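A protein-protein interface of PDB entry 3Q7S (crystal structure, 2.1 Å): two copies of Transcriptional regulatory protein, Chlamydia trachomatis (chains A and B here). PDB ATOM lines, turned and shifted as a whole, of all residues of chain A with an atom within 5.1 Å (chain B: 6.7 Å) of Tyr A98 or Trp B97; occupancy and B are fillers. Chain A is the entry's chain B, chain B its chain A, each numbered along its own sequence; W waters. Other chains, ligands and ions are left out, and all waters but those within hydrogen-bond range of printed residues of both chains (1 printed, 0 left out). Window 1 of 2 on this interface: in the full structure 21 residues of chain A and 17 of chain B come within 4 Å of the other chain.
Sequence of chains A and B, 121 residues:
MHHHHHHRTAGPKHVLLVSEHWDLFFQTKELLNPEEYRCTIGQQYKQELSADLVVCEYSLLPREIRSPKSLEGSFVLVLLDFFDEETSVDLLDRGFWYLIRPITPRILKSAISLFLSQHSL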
ATOM      1  N   LEU A  77       8.659 -22.603 -15.239  1.00  0.00           N
ATOM      2  CA  LEU A  77       7.682 -21.800 -15.912  1.00  0.00           C
ATOM      3  C   LEU A  77       7.867 -22.154 -17.369  1.00  0.00           C
ATOM      4  O   LEU A  77       9.002 -22.248 -17.836  1.00  0.00           O
ATOM      5  CB  LEU A  77       7.979 -20.331 -15.651  1.00  0.00           C
ATOM      6  CG  LEU A  77       7.092 -19.341 -16.418  1.00  0.00           C
ATOM      7  CD1 LEU A  77       5.625 -19.426 -15.971  1.00  0.00           C
ATOM      8  CD2 LEU A  77       7.666 -17.940 -16.217  1.00  0.00           C
ATOM      9  N   VAL A  78       6.764 -22.362 -18.085  1.00  0.00           N
ATOM     10  CA  VAL A  78       6.813 -22.919 -19.419  1.00  0.00           C
ATOM     11  C   VAL A  78       6.289 -21.879 -20.355  1.00  0.00           C
ATOM     12  O   VAL A  78       5.352 -21.195 -20.044  1.00  0.00           O
ATOM     13  CB  VAL A  78       5.973 -24.202 -19.515  1.00  0.00           C
ATOM     14  CG1 VAL A  78       5.878 -24.712 -20.964  1.00  0.00           C
ATOM     15  CG2 VAL A  78       6.574 -25.212 -18.570  1.00  0.00           C
ATOM     16  N   LEU A  80       4.712 -20.818 -23.898  1.00  0.00           N
ATOM     17  CA  LEU A  80       3.877 -21.418 -24.921  1.00  0.00           C
ATOM     18  C   LEU A  80       3.771 -20.468 -26.042  1.00  0.00           C
ATOM     19  O   LEU A  80       3.658 -19.272 -25.817  1.00  0.00           O
ATOM     20  CB  LEU A  80       2.466 -21.708 -24.400  1.00  0.00           C
ATOM     21  CG  LEU A  80       2.377 -22.967 -23.551  1.00  0.00           C
ATOM     22  CD1 LEU A  80       1.065 -22.945 -22.806  1.00  0.00           C
ATOM     23  CD2 LEU A  80       2.541 -24.233 -24.440  1.00  0.00           C
ATOM     24  N   SER A  88      -2.725 -26.736 -21.872  1.00  0.00           N
ATOM     25  CA  SER A  88      -2.785 -25.967 -20.629  1.00  0.00           C
ATOM     26  C   SER A  88      -3.181 -26.852 -19.465  1.00  0.00           C
ATOM     27  O   SER A  88      -2.545 -26.829 -18.416  1.00  0.00           O
ATOM     28  CB  SER A  88      -3.802 -24.831 -20.744  1.00  0.00           C
ATOM     29  OG  SER A  88      -3.525 -23.971 -21.837  1.00  0.00           O
ATOM     30  N   LEU A  91      -0.335 -29.191 -18.460  1.00  0.00           N
ATOM     31  CA  LEU A  91       0.813 -28.571 -17.788  1.00  0.00           C
ATOM     32  C   LEU A  91       0.503 -28.225 -16.360  1.00  0.00           C
ATOM     33  O   LEU A  91       1.296 -28.439 -15.456  1.00  0.00           O
ATOM     34  CB  LEU A  91       1.202 -27.271 -18.516  1.00  0.00           C
ATOM     35  CG  LEU A  91       1.913 -27.439 -19.838  1.00  0.00           C
ATOM     36  CD1 LEU A  91       2.041 -26.138 -20.635  1.00  0.00           C
ATOM     37  CD2 LEU A  91       3.281 -28.009 -19.529  1.00  0.00           C
ATOM     38  N   LEU A  92      -0.657 -27.633 -16.153  1.00  0.00           N
ATOM     39  CA  LEU A  92      -1.063 -27.338 -14.797  1.00  0.00           C
ATOM     40  C   LEU A  92      -1.137 -28.614 -13.929  1.00  0.00           C
ATOM     41  O   LEU A  92      -0.667 -28.613 -12.790  1.00  0.00           O
ATOM     42  CB  LEU A  92      -2.387 -26.595 -14.792  1.00  0.00           C
ATOM     43  CG  LEU A  92      -2.331 -25.223 -15.482  1.00  0.00           C
ATOM     44  CD1 LEU A  92      -3.791 -24.726 -15.718  1.00  0.00           C
ATOM     45  CD2 LEU A  92      -1.554 -24.332 -14.652  1.00  0.00           C
ATOM     46  N   PHE A  96       3.086 -27.357 -13.764  1.00  0.00           N
ATOM     47  CA  PHE A  96       3.781 -26.243 -14.432  1.00  0.00           C
ATOM     48  C   PHE A  96       2.878 -25.005 -14.687  1.00  0.00           C
ATOM     49  O   PHE A  96       1.878 -25.105 -15.372  1.00  0.00           O
ATOM     50  CB  PHE A  96       4.312 -26.671 -15.805  1.00  0.00           C
ATOM     51  CG  PHE A  96       5.291 -27.795 -15.755  1.00  0.00           C
ATOM     52  CD1 PHE A  96       6.602 -27.564 -15.373  1.00  0.00           C
ATOM     53  CD2 PHE A  96       4.914 -29.100 -16.118  1.00  0.00           C
ATOM     54  CE1 PHE A  96       7.518 -28.616 -15.324  1.00  0.00           C
ATOM     55  CE2 PHE A  96       5.833 -30.133 -16.065  1.00  0.00           C
ATOM     56  CZ  PHE A  96       7.131 -29.883 -15.667  1.00  0.00           C
ATOM     57  N   TRP A  97       3.254 -23.840 -14.183  1.00  0.00           N
ATOM     58  CA  TRP A  97       2.698 -22.585 -14.703  1.00  0.00           C
ATOM     59  C   TRP A  97       3.267 -22.207 -16.069  1.00  0.00           C
ATOM     60  O   TRP A  97       4.371 -22.644 -16.454  1.00  0.00           O
ATOM     61  CB  TRP A  97       2.975 -21.457 -13.746  1.00  0.00           C
ATOM     62  CG  TRP A  97       2.331 -21.639 -12.450  1.00  0.00           C
ATOM     63  CD1 TRP A  97       2.944 -21.977 -11.294  1.00  0.00           C
ATOM     64  CD2 TRP A  97       0.921 -21.511 -12.140  1.00  0.00           C
ATOM     65  NE1 TRP A  97       2.017 -22.061 -10.273  1.00  0.00           N
ATOM     66  CE2 TRP A  97       0.772 -21.773 -10.769  1.00  0.00           C
ATOM     67  CE3 TRP A  97      -0.212 -21.194 -12.884  1.00  0.00           C
ATOM     68  CZ2 TRP A  97      -0.463 -21.731 -10.123  1.00  0.00           C
ATOM     69  CZ3 TRP A  97      -1.456 -21.164 -12.229  1.00  0.00           C
ATOM     70  CH2 TRP A  97      -1.552 -21.420 -10.853  1.00  0.00           C
ATOM     71  N   TYR A  98       2.515 -21.400 -16.818  1.00  0.00           N
ATOM     72  CA  TYR A  98       2.943 -21.031 -18.148  1.00  0.00           C
ATOM     73  C   TYR A  98       2.635 -19.576 -18.512  1.00  0.00           C
ATOM     74  O   TYR A  98       1.762 -18.971 -17.912  1.00  0.00           O
ATOM     75  CB  TYR A  98       2.294 -21.931 -19.188  1.00  0.00           C
ATOM     76  CG  TYR A  98       0.798 -21.975 -19.147  1.00  0.00           C
ATOM     77  CD1 TYR A  98       0.044 -21.006 -19.741  1.00  0.00           C
ATOM     78  CD2 TYR A  98       0.132 -23.038 -18.516  1.00  0.00           C
ATOM     79  CE1 TYR A  98      -1.341 -21.035 -19.689  1.00  0.00           C
ATOM     80  CE2 TYR A  98      -1.246 -23.080 -18.457  1.00  0.00           C
ATOM     81  CZ  TYR A  98      -1.984 -22.095 -19.047  1.00  0.00           C
ATOM     82  OH  TYR A  98      -3.358 -22.173 -19.017  1.00  0.00           O
ATOM     83  N   LEU A  99       3.367 -19.054 -19.499  1.00  0.00           N
ATOM     84  CA  LEU A  99       2.995 -17.839 -20.189  1.00  0.00           C
ATOM     85  C   LEU A  99       2.776 -18.233 -21.602  1.00  0.00           C
ATOM     86  O   LEU A  99       3.477 -19.104 -22.094  1.00  0.00           O
ATOM     87  CB  LEU A  99       4.135 -16.819 -20.171  1.00  0.00           C
ATOM     88  CG  LEU A  99       4.430 -16.303 -18.783  1.00  0.00           C
ATOM     89  CD1 LEU A  99       5.638 -15.493 -18.833  1.00  0.00           C
ATOM     90  CD2 LEU A  99       3.230 -15.496 -18.221  1.00  0.00           C
ATOM     91  N   ILE A 100       1.822 -17.590 -22.265  1.00  0.00           N
ATOM     92  CA  ILE A 100       1.594 -17.775 -23.687  1.00  0.00           C
ATOM     93  C   ILE A 100       2.082 -16.513 -24.439  1.00  0.00           C
ATOM     94  O   ILE A 100       1.960 -15.424 -23.928  1.00  0.00           O
ATOM     95  CB  ILE A 100       0.094 -18.026 -23.933  1.00  0.00           C
ATOM     96  CG1 ILE A 100      -0.327 -19.348 -23.266  1.00  0.00           C
ATOM     97  CG2 ILE A 100      -0.243 -18.055 -25.446  1.00  0.00           C
ATOM     98  CD1 ILE A 100      -1.745 -19.663 -23.432  1.00  0.00           C
ATOM     99  N   ALA A 111       8.084 -11.776 -14.495  1.00  0.00           N
ATOM    100  CA  ALA A 111       7.554 -13.108 -14.110  1.00  0.00           C
ATOM    101  C   ALA A 111       8.631 -13.782 -13.247  1.00  0.00           C
ATOM    102  O   ALA A 111       8.386 -14.168 -12.139  1.00  0.00           O
ATOM    103  CB  ALA A 111       7.250 -13.919 -15.332  1.00  0.00           C
ATOM    104  N   LEU A 114       8.837 -12.249  -9.881  1.00  0.00           N
ATOM    105  CA  LEU A 114       7.689 -12.670  -9.095  1.00  0.00           C
ATOM    106  C   LEU A 114       7.849 -14.108  -8.564  1.00  0.00           C
ATOM    107  O   LEU A 114       7.613 -14.386  -7.391  1.00  0.00           O
ATOM    108  CB  LEU A 114       6.410 -12.596  -9.914  1.00  0.00           C
ATOM    109  CG  LEU A 114       5.219 -13.125  -9.085  1.00  0.00           C
ATOM    110  CD1 LEU A 114       4.879 -12.128  -7.999  1.00  0.00           C
ATOM    111  CD2 LEU A 114       3.979 -13.372  -9.861  1.00  0.00           C
ATOM    112  N   PHE A 115       8.216 -15.033  -9.432  1.00  0.00           N
ATOM    113  CA  PHE A 115       8.334 -16.440  -9.023  1.00  0.00           C
ATOM    114  C   PHE A 115       9.396 -16.608  -7.944  1.00  0.00           C
ATOM    115  O   PHE A 115       9.236 -17.375  -7.016  1.00  0.00           O
ATOM    116  CB  PHE A 115       8.677 -17.307 -10.227  1.00  0.00           C
ATOM    117  CG  PHE A 115       7.468 -17.830 -10.971  1.00  0.00           C
ATOM    118  CD1 PHE A 115       6.461 -16.950 -11.410  1.00  0.00           C
ATOM    119  CD2 PHE A 115       7.336 -19.212 -11.238  1.00  0.00           C
ATOM    120  CE1 PHE A 115       5.350 -17.433 -12.113  1.00  0.00           C
ATOM    121  CE2 PHE A 115       6.225 -19.719 -11.932  1.00  0.00           C
ATOM    122  CZ  PHE A 115       5.228 -18.827 -12.378  1.00  0.00           C
ATOM    123  N   VAL B  76      -3.939 -13.980  -4.269  1.00  0.00           N
ATOM    124  CA  VAL B  76      -4.919 -13.581  -5.230  1.00  0.00           C
ATOM    125  C   VAL B  76      -4.355 -13.986  -6.568  1.00  0.00           C
ATOM    126  O   VAL B  76      -3.216 -13.713  -6.849  1.00  0.00           O
ATOM    127  CB  VAL B  76      -5.171 -12.067  -5.203  1.00  0.00           C
ATOM    128  CG1 VAL B  76      -6.013 -11.595  -6.428  1.00  0.00           C
ATOM    129  CG2 VAL B  76      -5.874 -11.681  -3.937  1.00  0.00           C
ATOM    130  N   LEU B  77      -5.164 -14.668  -7.362  1.00  0.00           N
ATOM    131  CA  LEU B  77      -4.833 -15.010  -8.729  1.00  0.00           C
ATOM    132  C   LEU B  77      -5.809 -14.210  -9.607  1.00  0.00           C
ATOM    133  O   LEU B  77      -6.972 -14.070  -9.282  1.00  0.00           O
ATOM    134  CB  LEU B  77      -5.040 -16.522  -8.950  1.00  0.00           C
ATOM    135  CG  LEU B  77      -5.068 -17.071 -10.393  1.00  0.00           C
ATOM    136  CD1 LEU B  77      -3.664 -17.043 -10.970  1.00  0.00           C
ATOM    137  CD2 LEU B  77      -5.605 -18.507 -10.384  1.00  0.00           C
ATOM    138  N   VAL B  78      -5.329 -13.676 -10.708  1.00  0.00           N
ATOM    139  CA  VAL B  78      -6.148 -12.761 -11.505  1.00  0.00           C
ATOM    140  C   VAL B  78      -6.456 -13.321 -12.886  1.00  0.00           C
ATOM    141  O   VAL B  78      -5.605 -13.923 -13.522  1.00  0.00           O
ATOM    142  CB  VAL B  78      -5.394 -11.370 -11.623  1.00  0.00           C
ATOM    143  CG1 VAL B  78      -5.969 -10.527 -12.732  1.00  0.00           C
ATOM    144  CG2 VAL B  78      -5.435 -10.641 -10.317  1.00  0.00           C
ATOM    145  N   LEU B  79      -7.698 -13.131 -13.328  1.00  0.00           N
ATOM    146  CA  LEU B  79      -8.174 -13.542 -14.640  1.00  0.00           C
ATOM    147  C   LEU B  79      -8.317 -12.303 -15.522  1.00  0.00           C
ATOM    148  O   LEU B  79      -9.081 -11.423 -15.190  1.00  0.00           O
ATOM    149  CB  LEU B  79      -9.589 -14.129 -14.492  1.00  0.00           C
ATOM    150  CG  LEU B  79      -9.722 -15.332 -13.520  1.00  0.00           C
ATOM    151  CD1 LEU B  79     -11.098 -16.038 -13.649  1.00  0.00           C
ATOM    152  CD2 LEU B  79      -8.521 -16.343 -13.707  1.00  0.00           C
ATOM    153  N   LEU B  91       0.625  -6.148 -13.327  1.00  0.00           N
ATOM    154  CA  LEU B  91       0.141  -7.160 -12.418  1.00  0.00           C
ATOM    155  C   LEU B  91       1.300  -7.901 -11.767  1.00  0.00           C
ATOM    156  O   LEU B  91       1.275  -8.139 -10.582  1.00  0.00           O
ATOM    157  CB  LEU B  91      -0.763  -8.170 -13.108  1.00  0.00           C
ATOM    158  CG  LEU B  91      -2.188  -7.742 -13.412  1.00  0.00           C
ATOM    159  CD1 LEU B  91      -2.885  -8.777 -14.374  1.00  0.00           C
ATOM    160  CD2 LEU B  91      -2.942  -7.576 -12.064  1.00  0.00           C
ATOM    161  N   LEU B  92       2.283  -8.307 -12.551  1.00  0.00           N
ATOM    162  CA  LEU B  92       3.380  -9.062 -12.012  1.00  0.00           C
ATOM    163  C   LEU B  92       4.142  -8.237 -10.957  1.00  0.00           C
ATOM    164  O   LEU B  92       4.400  -8.748  -9.907  1.00  0.00           O
ATOM    165  CB  LEU B  92       4.316  -9.577 -13.095  1.00  0.00           C
ATOM    166  CG  LEU B  92       3.726 -10.597 -14.083  1.00  0.00           C
ATOM    167  CD1 LEU B  92       4.651 -10.648 -15.358  1.00  0.00           C
ATOM    168  CD2 LEU B  92       3.419 -12.032 -13.450  1.00  0.00           C
ATOM    169  N   GLY B  95       2.538  -8.065  -7.683  1.00  0.00           N
ATOM    170  CA  GLY B  95       2.547  -9.357  -6.993  1.00  0.00           C
ATOM    171  C   GLY B  95       1.428 -10.335  -7.344  1.00  0.00           C
ATOM    172  O   GLY B  95       1.208 -11.319  -6.642  1.00  0.00           O
ATOM    173  N   PHE B  96       0.729 -10.100  -8.438  1.00  0.00           N
ATOM    174  CA  PHE B  96      -0.299 -11.016  -8.907  1.00  0.00           C
ATOM    175  C   PHE B  96       0.158 -11.801 -10.115  1.00  0.00           C
ATOM    176  O   PHE B  96       0.573 -11.236 -11.132  1.00  0.00           O
ATOM    177  CB  PHE B  96      -1.542 -10.228  -9.317  1.00  0.00           C
ATOM    178  CG  PHE B  96      -2.027  -9.274  -8.247  1.00  0.00           C
ATOM    179  CD1 PHE B  96      -2.743  -9.748  -7.148  1.00  0.00           C
ATOM    180  CD2 PHE B  96      -1.765  -7.907  -8.335  1.00  0.00           C
ATOM    181  CE1 PHE B  96      -3.188  -8.885  -6.130  1.00  0.00           C
ATOM    182  CE2 PHE B  96      -2.229  -7.054  -7.332  1.00  0.00           C
ATOM    183  CZ  PHE B  96      -2.944  -7.533  -6.234  1.00  0.00           C
ATOM    184  N   TRP B  97       0.037 -13.114 -10.005  1.00  0.00           N
ATOM    185  CA  TRP B  97       0.108 -13.995 -11.135  1.00  0.00           C
ATOM    186  C   TRP B  97      -1.302 -13.988 -11.733  1.00  0.00           C
ATOM    187  O   TRP B  97      -2.270 -13.640 -11.042  1.00  0.00           O
ATOM    188  CB  TRP B  97       0.533 -15.390 -10.626  1.00  0.00           C
ATOM    189  CG  TRP B  97       0.723 -16.439 -11.716  1.00  0.00           C
ATOM    190  CD1 TRP B  97       0.125 -17.681 -11.809  1.00  0.00           C
ATOM    191  CD2 TRP B  97       1.596 -16.332 -12.858  1.00  0.00           C
ATOM    192  NE1 TRP B  97       0.581 -18.339 -12.933  1.00  0.00           N
ATOM    193  CE2 TRP B  97       1.469 -17.534 -13.599  1.00  0.00           C
ATOM    194  CE3 TRP B  97       2.470 -15.339 -13.320  1.00  0.00           C
ATOM    195  CZ2 TRP B  97       2.179 -17.765 -14.778  1.00  0.00           C
ATOM    196  CZ3 TRP B  97       3.182 -15.569 -14.509  1.00  0.00           C
ATOM    197  CH2 TRP B  97       3.032 -16.778 -15.222  1.00  0.00           C
ATOM    198  N   TYR B  98      -1.432 -14.405 -12.991  1.00  0.00           N
ATOM    199  CA  TYR B  98      -2.685 -14.325 -13.696  1.00  0.00           C
ATOM    200  C   TYR B  98      -2.827 -15.409 -14.774  1.00  0.00           C
ATOM    201  O   TYR B  98      -1.865 -16.005 -15.204  1.00  0.00           O
ATOM    202  CB  TYR B  98      -2.794 -12.947 -14.360  1.00  0.00           C
ATOM    203  CG  TYR B  98      -1.635 -12.648 -15.280  1.00  0.00           C
ATOM    204  CD1 TYR B  98      -1.614 -13.149 -16.581  1.00  0.00           C
ATOM    205  CD2 TYR B  98      -0.538 -11.858 -14.842  1.00  0.00           C
ATOM    206  CE1 TYR B  98      -0.517 -12.870 -17.443  1.00  0.00           C
ATOM    207  CE2 TYR B  98       0.530 -11.596 -15.680  1.00  0.00           C
ATOM    208  CZ  TYR B  98       0.541 -12.094 -16.974  1.00  0.00           C
ATOM    209  OH  TYR B  98       1.617 -11.841 -17.799  1.00  0.00           O
ATOM    210  N   LEU B  99      -4.045 -15.611 -15.232  1.00  0.00           N
ATOM    211  CA  LEU B  99      -4.281 -16.273 -16.496  1.00  0.00           C
ATOM    212  C   LEU B  99      -4.995 -15.334 -17.459  1.00  0.00           C
ATOM    213  O   LEU B  99      -5.881 -14.601 -17.075  1.00  0.00           O
ATOM    214  CB  LEU B  99      -5.204 -17.493 -16.285  1.00  0.00           C
ATOM    215  CG  LEU B  99      -4.859 -18.476 -15.160  1.00  0.00           C
ATOM    216  CD1 LEU B  99      -6.009 -19.478 -14.967  1.00  0.00           C
ATOM    217  CD2 LEU B  99      -3.638 -19.244 -15.494  1.00  0.00           C
ATOM    218  N   ILE B 100      -4.639 -15.411 -18.734  1.00  0.00           N
ATOM    219  CA  ILE B 100      -5.363 -14.716 -19.750  1.00  0.00           C
ATOM    220  C   ILE B 100      -6.349 -15.630 -20.431  1.00  0.00           C
ATOM    221  O   ILE B 100      -6.021 -16.800 -20.633  1.00  0.00           O
ATOM    222  CB  ILE B 100      -4.376 -14.110 -20.757  1.00  0.00           C
ATOM    223  CG1 ILE B 100      -3.468 -13.127 -19.985  1.00  0.00           C
ATOM    224  CG2 ILE B 100      -5.140 -13.479 -21.935  1.00  0.00           C
ATOM    225  CD1 ILE B 100      -2.389 -12.532 -20.747  1.00  0.00           C
ATOM    226  N   PRO B 102      -8.588 -17.483 -23.342  1.00  0.00           N
ATOM    227  CA  PRO B 102      -9.636 -18.404 -22.894  1.00  0.00           C
ATOM    228  C   PRO B 102      -9.399 -19.101 -21.564  1.00  0.00           C
ATOM    229  O   PRO B 102      -8.393 -19.766 -21.392  1.00  0.00           O
ATOM    230  CB  PRO B 102      -9.693 -19.421 -24.061  1.00  0.00           C
ATOM    231  CG  PRO B 102      -9.384 -18.572 -25.225  1.00  0.00           C
ATOM    232  CD  PRO B 102      -8.216 -17.780 -24.744  1.00  0.00           C
ATOM    233  N   ILE B 107      -9.375 -25.535 -17.053  1.00  0.00           N
ATOM    234  CA  ILE B 107      -8.207 -24.705 -16.765  1.00  0.00           C
ATOM    235  C   ILE B 107      -8.306 -24.117 -15.355  1.00  0.00           C
ATOM    236  O   ILE B 107      -7.395 -24.217 -14.538  1.00  0.00           O
ATOM    237  CB  ILE B 107      -8.077 -23.618 -17.850  1.00  0.00           C
ATOM    238  CG1 ILE B 107      -7.824 -24.307 -19.204  1.00  0.00           C
ATOM    239  CG2 ILE B 107      -6.942 -22.578 -17.498  1.00  0.00           C
ATOM    240  CD1 ILE B 107      -7.714 -23.415 -20.311  1.00  0.00           C
ATOM    241  N   PHE B 115      -2.207 -23.886  -7.621  1.00  0.00           N
ATOM    242  CA  PHE B 115      -1.806 -22.765  -6.841  1.00  0.00           C
ATOM    243  C   PHE B 115      -1.777 -23.138  -5.369  1.00  0.00           C
ATOM    244  O   PHE B 115      -0.813 -22.888  -4.653  1.00  0.00           O
ATOM    245  CB  PHE B 115      -2.782 -21.636  -7.071  1.00  0.00           C
ATOM    246  CG  PHE B 115      -2.275 -20.337  -6.599  1.00  0.00           C
ATOM    247  CD1 PHE B 115      -1.853 -19.387  -7.510  1.00  0.00           C
ATOM    248  CD2 PHE B 115      -2.199 -20.062  -5.253  1.00  0.00           C
ATOM    249  CE1 PHE B 115      -1.373 -18.172  -7.094  1.00  0.00           C
ATOM    250  CE2 PHE B 115      -1.712 -18.858  -4.821  1.00  0.00           C
ATOM    251  CZ  PHE B 115      -1.281 -17.915  -5.739  1.00  0.00           C
HETATM  252  O   HOH W   1      -0.752 -17.851 -16.969  1.00  0.00           O
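Water W1 bridges O of Tyr B98 (2.8 Å) and O of Tyr A98 (2.9 Å).
Of the 15 printed residues of chain B, 5 touch a printed residue of chain A.
Printed residues of chain B that touch a printed residue of chain A: Leu B92, Gly B95, Trp B97, Ile B107 and Phe B115.
Hydrophobic or aromatic side chains of chain B within 4 Å of the printed part of chain A: Leu B92, Trp B97, Ile B107 and Phe B115.
Hydrophobic or aromatic side chains of chain A within 4 Å of the printed part of chain B: Leu A77, Leu A92, Trp A97, Tyr A98, Leu A99, Leu A114 and Phe A115.
Among the printed residues, 12 pairs touch across the chains.
Among the printed residues, no Asp or Glu carboxylate lies within 4 Å of a Lys or Arg side-chain nitrogen of the other chain.
The backbone NH of Leu A99 sits at hydrogen-bond distance from the backbone carbonyl oxygen of Val A78 (3.0 Å).
The backbone NH (N) of Val B78 sits at hydrogen-bond distance from the backbone carbonyl oxygen (O) of Trp B97 (3.1 Å).
The side-chain hydroxyl of Ser A88 sits close to the side-chain hydroxyl of Tyr A98, 3.3 Å away.
The backbone carbonyl oxygen (O) of Trp A97 sits at hydrogen-bond distance from the backbone NH (N) of Val A78 (2.9 Å).
The backbone NH (N) of Leu A80 lies within hydrogen-bond range of the backbone carbonyl oxygen (O) of Leu A99, at 2.8 Å.
CD1 of Leu A77 touches CH2 of Trp B97 (3.8 Å).
Leu A92 touches Ile B107.
Trp A97 touches Trp B97.
Trp A97 touches Phe B115 (CZ2 to CA, 3.7 Å).
Tyr A98 touches Trp B97.
Ile B107 touches Tyr A98.
CD1 of Leu B92 touches N of Ala A111, at 3.7 Å.
CD1 of Leu A114 touches CA of Gly B95 (3.8 Å).
Trp B97 touches Leu A114 (N to CD2, 3.95 Å).
CE1 of Phe A115 touches CZ3 of Trp B97, at 3.7 Å.
Trp A97 touches its own counterpart, Trp B97.
Trp A97 touches Phe B115, and with the chains exchanged Phe A115 touches Trp B97.
Tyr A98 touches Trp B97, but with the chains exchanged Trp A97 does not touch Tyr B98 (5.9 Å).
Leu A99 touches Trp B97, but with the chains exchanged Trp A97 does not touch Leu B99 (4.4 Å).
Tyr A98 touches just these residues of chain B: Trp B97 (3.4 Å) and Ile B107 (3.9 Å).
Trp B97 touches six residues of chain A.
Printed residues of chain B within 4 Å of Leu A92: Ile B107.
Printed residues of chain B within 4 Å of Trp A97: Trp B97 (3.0 Å) and Phe B115 (3.7 Å).
The nearest printed residue of chain B that does not touch Trp A97 is Leu B99 (4.4 Å).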
